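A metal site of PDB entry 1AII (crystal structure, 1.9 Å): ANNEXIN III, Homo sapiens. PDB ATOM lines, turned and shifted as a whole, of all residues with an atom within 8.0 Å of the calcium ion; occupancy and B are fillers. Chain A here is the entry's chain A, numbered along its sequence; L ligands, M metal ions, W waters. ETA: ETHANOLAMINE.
Within 4 Å of the calcium ion: Gly 186, Arg 189, Gly 191 and Glu 231.
The nearest printed residue that does not touch the calcium ion is Trp 190 (4.2 Å).
The calcium ion is bound by O of Gly 191 (2.4 Å), O of Arg 189 (2.6 Å), OE1 of Glu 231 (2.6 Å), O of Gly 186 (2.6 Å), water W2 (2.7 Å), water W1 (2.7 Å) and OE2 of Glu 231 (2.8 Å).
The calcium ion has seven donor atoms within binding distance.
The backbone NH of Glu 187 lies close to the side-chain carboxylate of Glu 231 (3.5 Å).
The side-chain hydroxyl (OG1) of Thr 192 sits close to the side-chain carboxylate (OE1) of Glu 231.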
ATOM      1  N   LEU A 182     -18.992   2.066  -2.156  1.00  0.00           N
ATOM      2  CA  LEU A 182     -18.066   1.135  -1.496  1.00  0.00           C
ATOM      3  C   LEU A 182     -18.857  -0.101  -1.047  1.00  0.00           C
ATOM      4  O   LEU A 182     -18.452  -1.250  -1.174  1.00  0.00           O
ATOM      5  CB  LEU A 182     -17.376   1.785  -0.300  1.00  0.00           C
ATOM      6  CG  LEU A 182     -16.222   2.784  -0.534  1.00  0.00           C
ATOM      7  CD1 LEU A 182     -15.657   3.279   0.791  1.00  0.00           C
ATOM      8  CD2 LEU A 182     -15.121   2.178  -1.391  1.00  0.00           C
ATOM      9  N   TYR A 183     -20.020   0.139  -0.458  1.00  0.00           N
ATOM     10  CA  TYR A 183     -20.900  -0.923   0.027  1.00  0.00           C
ATOM     11  C   TYR A 183     -21.313  -1.839  -1.125  1.00  0.00           C
ATOM     12  O   TYR A 183     -21.256  -3.063  -0.969  1.00  0.00           O
ATOM     13  CB  TYR A 183     -22.134  -0.377   0.737  1.00  0.00           C
ATOM     14  CG  TYR A 183     -23.009  -1.435   1.363  1.00  0.00           C
ATOM     15  CD1 TYR A 183     -22.605  -2.106   2.520  1.00  0.00           C
ATOM     16  CD2 TYR A 183     -24.245  -1.768   0.825  1.00  0.00           C
ATOM     17  CE1 TYR A 183     -23.401  -3.065   3.102  1.00  0.00           C
ATOM     18  CE2 TYR A 183     -25.050  -2.744   1.395  1.00  0.00           C
ATOM     19  CZ  TYR A 183     -24.626  -3.396   2.537  1.00  0.00           C
ATOM     20  OH  TYR A 183     -25.422  -4.368   3.104  1.00  0.00           O
ATOM     21  N   LYS A 184     -21.712  -1.316  -2.263  1.00  0.00           N
ATOM     22  CA  LYS A 184     -22.125  -2.086  -3.421  1.00  0.00           C
ATOM     23  C   LYS A 184     -20.949  -2.821  -4.050  1.00  0.00           C
ATOM     24  O   LYS A 184     -21.145  -3.900  -4.606  1.00  0.00           O
ATOM     25  CB  LYS A 184     -22.740  -1.221  -4.534  1.00  0.00           C
ATOM     26  CG  LYS A 184     -24.128  -0.695  -4.227  1.00  0.00           C
ATOM     27  CD  LYS A 184     -24.765   0.027  -5.416  1.00  0.00           C
ATOM     28  CE  LYS A 184     -25.889   0.930  -4.942  1.00  0.00           C
ATOM     29  NZ  LYS A 184     -26.144   2.082  -5.863  1.00  0.00           N
ATOM     30  N   ALA A 185     -19.759  -2.227  -3.968  1.00  0.00           N
ATOM     31  CA  ALA A 185     -18.554  -2.792  -4.531  1.00  0.00           C
ATOM     32  C   ALA A 185     -17.938  -3.960  -3.778  1.00  0.00           C
ATOM     33  O   ALA A 185     -17.138  -4.718  -4.324  1.00  0.00           O
ATOM     34  CB  ALA A 185     -17.489  -1.667  -4.571  1.00  0.00           C
ATOM     35  N   GLY A 186     -18.295  -4.100  -2.523  1.00  0.00           N
ATOM     36  CA  GLY A 186     -17.802  -5.115  -1.637  1.00  0.00           C
ATOM     37  C   GLY A 186     -18.891  -5.874  -0.912  1.00  0.00           C
ATOM     38  O   GLY A 186     -19.398  -6.831  -1.469  1.00  0.00           O
ATOM     39  N   GLU A 187     -19.296  -5.531   0.275  1.00  0.00           N
ATOM     40  CA  GLU A 187     -20.297  -6.210   1.051  1.00  0.00           C
ATOM     41  C   GLU A 187     -21.531  -6.670   0.306  1.00  0.00           C
ATOM     42  O   GLU A 187     -21.944  -7.807   0.491  1.00  0.00           O
ATOM     43  CB  GLU A 187     -20.783  -5.320   2.221  1.00  0.00           C
ATOM     44  CG  GLU A 187     -19.700  -5.024   3.233  1.00  0.00           C
ATOM     45  CD  GLU A 187     -19.302  -6.197   4.108  1.00  0.00           C
ATOM     46  OE1 GLU A 187     -19.950  -7.262   4.126  1.00  0.00           O
ATOM     47  OE2 GLU A 187     -18.318  -6.088   4.846  1.00  0.00           O
ATOM     48  N   ASN A 188     -22.132  -5.804  -0.493  1.00  0.00           N
ATOM     49  CA  ASN A 188     -23.340  -6.143  -1.209  1.00  0.00           C
ATOM     50  C   ASN A 188     -23.219  -7.032  -2.421  1.00  0.00           C
ATOM     51  O   ASN A 188     -24.280  -7.326  -3.003  1.00  0.00           O
ATOM     52  CB  ASN A 188     -24.031  -4.816  -1.600  1.00  0.00           C
ATOM     53  CG  ASN A 188     -25.539  -4.990  -1.776  1.00  0.00           C
ATOM     54  OD1 ASN A 188     -26.044  -4.708  -2.867  1.00  0.00           O
ATOM     55  ND2 ASN A 188     -26.209  -5.459  -0.730  1.00  0.00           N
ATOM     56  N   ARG A 189     -22.073  -7.493  -2.862  1.00  0.00           N
ATOM     57  CA  ARG A 189     -22.082  -8.354  -4.046  1.00  0.00           C
ATOM     58  C   ARG A 189     -21.223  -9.577  -3.885  1.00  0.00           C
ATOM     59  O   ARG A 189     -20.457  -9.580  -2.936  1.00  0.00           O
ATOM     60  CB  ARG A 189     -21.522  -7.559  -5.237  1.00  0.00           C
ATOM     61  CG  ARG A 189     -20.167  -6.911  -4.990  1.00  0.00           C
ATOM     62  CD  ARG A 189     -19.555  -6.491  -6.310  1.00  0.00           C
ATOM     63  NE  ARG A 189     -18.900  -7.611  -6.970  1.00  0.00           N
ATOM     64  CZ  ARG A 189     -18.299  -7.610  -8.145  1.00  0.00           C
ATOM     65  NH1 ARG A 189     -18.244  -6.503  -8.883  1.00  0.00           N
ATOM     66  NH2 ARG A 189     -17.741  -8.721  -8.617  1.00  0.00           N
ATOM     67  N   TRP A 190     -21.306 -10.571  -4.748  1.00  0.00           N
ATOM     68  CA  TRP A 190     -20.442 -11.740  -4.634  1.00  0.00           C
ATOM     69  C   TRP A 190     -19.080 -11.216  -5.133  1.00  0.00           C
ATOM     70  O   TRP A 190     -19.073 -10.458  -6.112  1.00  0.00           O
ATOM     71  CB  TRP A 190     -20.910 -12.915  -5.503  1.00  0.00           C
ATOM     72  CG  TRP A 190     -22.217 -13.501  -5.055  1.00  0.00           C
ATOM     73  CD1 TRP A 190     -22.825 -13.363  -3.854  1.00  0.00           C
ATOM     74  CD2 TRP A 190     -23.072 -14.343  -5.842  1.00  0.00           C
ATOM     75  NE1 TRP A 190     -24.010 -14.040  -3.839  1.00  0.00           N
ATOM     76  CE2 TRP A 190     -24.179 -14.651  -5.052  1.00  0.00           C
ATOM     77  CE3 TRP A 190     -22.982 -14.836  -7.152  1.00  0.00           C
ATOM     78  CZ2 TRP A 190     -25.237 -15.457  -5.504  1.00  0.00           C
ATOM     79  CZ3 TRP A 190     -24.018 -15.635  -7.597  1.00  0.00           C
ATOM     80  CH2 TRP A 190     -25.115 -15.943  -6.780  1.00  0.00           C
ATOM     81  N   GLY A 191     -17.953 -11.600  -4.514  1.00  0.00           N
ATOM     82  CA  GLY A 191     -16.734 -11.007  -5.034  1.00  0.00           C
ATOM     83  C   GLY A 191     -16.574  -9.564  -4.628  1.00  0.00           C
ATOM     84  O   GLY A 191     -17.254  -9.078  -3.721  1.00  0.00           O
ATOM     85  N   THR A 192     -15.687  -8.848  -5.292  1.00  0.00           N
ATOM     86  CA  THR A 192     -15.447  -7.452  -4.977  1.00  0.00           C
ATOM     87  C   THR A 192     -15.045  -6.638  -6.198  1.00  0.00           C
ATOM     88  O   THR A 192     -14.345  -7.145  -7.075  1.00  0.00           O
ATOM     89  CB  THR A 192     -14.292  -7.299  -3.948  1.00  0.00           C
ATOM     90  OG1 THR A 192     -14.484  -8.213  -2.877  1.00  0.00           O
ATOM     91  CG2 THR A 192     -14.221  -5.871  -3.425  1.00  0.00           C
ATOM     92  N   ASP A 193     -15.508  -5.409  -6.283  1.00  0.00           N
ATOM     93  CA  ASP A 193     -15.054  -4.537  -7.356  1.00  0.00           C
ATOM     94  C   ASP A 193     -13.838  -3.771  -6.844  1.00  0.00           C
ATOM     95  O   ASP A 193     -13.951  -2.606  -6.480  1.00  0.00           O
ATOM     96  CB  ASP A 193     -16.171  -3.602  -7.838  1.00  0.00           C
ATOM     97  CG  ASP A 193     -15.742  -2.800  -9.061  1.00  0.00           C
ATOM     98  OD1 ASP A 193     -14.530  -2.831  -9.395  1.00  0.00           O
ATOM     99  OD2 ASP A 193     -16.597  -2.141  -9.675  1.00  0.00           O
ATOM    100  N   PHE A 197     -12.667   0.267  -5.037  1.00  0.00           N
ATOM    101  CA  PHE A 197     -12.039   0.500  -3.738  1.00  0.00           C
ATOM    102  C   PHE A 197     -10.807   1.382  -3.965  1.00  0.00           C
ATOM    103  O   PHE A 197     -10.582   2.359  -3.270  1.00  0.00           O
ATOM    104  CB  PHE A 197     -11.655  -0.793  -3.011  1.00  0.00           C
ATOM    105  CG  PHE A 197     -12.744  -1.340  -2.124  1.00  0.00           C
ATOM    106  CD1 PHE A 197     -13.795  -2.087  -2.638  1.00  0.00           C
ATOM    107  CD2 PHE A 197     -12.737  -1.087  -0.754  1.00  0.00           C
ATOM    108  CE1 PHE A 197     -14.777  -2.570  -1.791  1.00  0.00           C
ATOM    109  CE2 PHE A 197     -13.725  -1.564   0.087  1.00  0.00           C
ATOM    110  CZ  PHE A 197     -14.754  -2.309  -0.428  1.00  0.00           C
ATOM    111  N   SER A 227     -14.790  -4.366   6.423  1.00  0.00           N
ATOM    112  CA  SER A 227     -15.171  -4.737   5.059  1.00  0.00           C
ATOM    113  C   SER A 227     -13.928  -5.038   4.235  1.00  0.00           C
ATOM    114  O   SER A 227     -13.890  -5.981   3.448  1.00  0.00           O
ATOM    115  CB  SER A 227     -16.034  -3.672   4.391  1.00  0.00           C
ATOM    116  OG  SER A 227     -17.284  -3.523   5.043  1.00  0.00           O
ATOM    117  N   GLY A 230     -12.781  -8.314   5.214  1.00  0.00           N
ATOM    118  CA  GLY A 230     -13.503  -9.500   4.797  1.00  0.00           C
ATOM    119  C   GLY A 230     -13.561  -9.646   3.297  1.00  0.00           C
ATOM    120  O   GLY A 230     -13.831 -10.737   2.777  1.00  0.00           O
ATOM    121  N   GLU A 231     -13.293  -8.558   2.576  1.00  0.00           N
ATOM    122  CA  GLU A 231     -13.381  -8.552   1.119  1.00  0.00           C
ATOM    123  C   GLU A 231     -12.057  -8.786   0.408  1.00  0.00           C
ATOM    124  O   GLU A 231     -11.993  -9.467  -0.613  1.00  0.00           O
ATOM    125  CB  GLU A 231     -13.903  -7.216   0.604  1.00  0.00           C
ATOM    126  CG  GLU A 231     -15.334  -6.925   0.977  1.00  0.00           C
ATOM    127  CD  GLU A 231     -16.314  -7.770   0.193  1.00  0.00           C
ATOM    128  OE1 GLU A 231     -16.128  -7.917  -1.030  1.00  0.00           O
ATOM    129  OE2 GLU A 231     -17.272  -8.292   0.811  1.00  0.00           O
ATOM    130  N   LEU A 232     -10.982  -8.215   0.927  1.00  0.00           N
ATOM    131  CA  LEU A 232      -9.696  -8.314   0.247  1.00  0.00           C
ATOM    132  C   LEU A 232      -8.689  -9.122   1.052  1.00  0.00           C
ATOM    133  O   LEU A 232      -8.972  -9.584   2.147  1.00  0.00           O
ATOM    134  CB  LEU A 232      -9.209  -6.906  -0.062  1.00  0.00           C
ATOM    135  CG  LEU A 232     -10.284  -5.928  -0.567  1.00  0.00           C
ATOM    136  CD1 LEU A 232      -9.937  -4.490  -0.194  1.00  0.00           C
ATOM    137  CD2 LEU A 232     -10.473  -6.064  -2.063  1.00  0.00           C
HETATM  138  CA  ETA L   1     -14.547 -11.625  -7.182  1.00  0.00           C
HETATM  139  N   ETA L   1     -15.404 -11.539  -8.398  1.00  0.00           N
HETATM  140  C   ETA L   1     -13.960 -13.004  -7.009  1.00  0.00           C
HETATM  141  O   ETA L   1     -14.031 -13.696  -8.244  1.00  0.00           O
HETATM  142 CA    CA M   1     -18.319  -9.217  -1.568  1.00  0.00          CA
HETATM  143  O   HOH W   1     -20.198 -10.067   0.184  1.00  0.00           O
HETATM  144  O   HOH W   2     -16.890 -11.465  -1.285  1.00  0.00           O
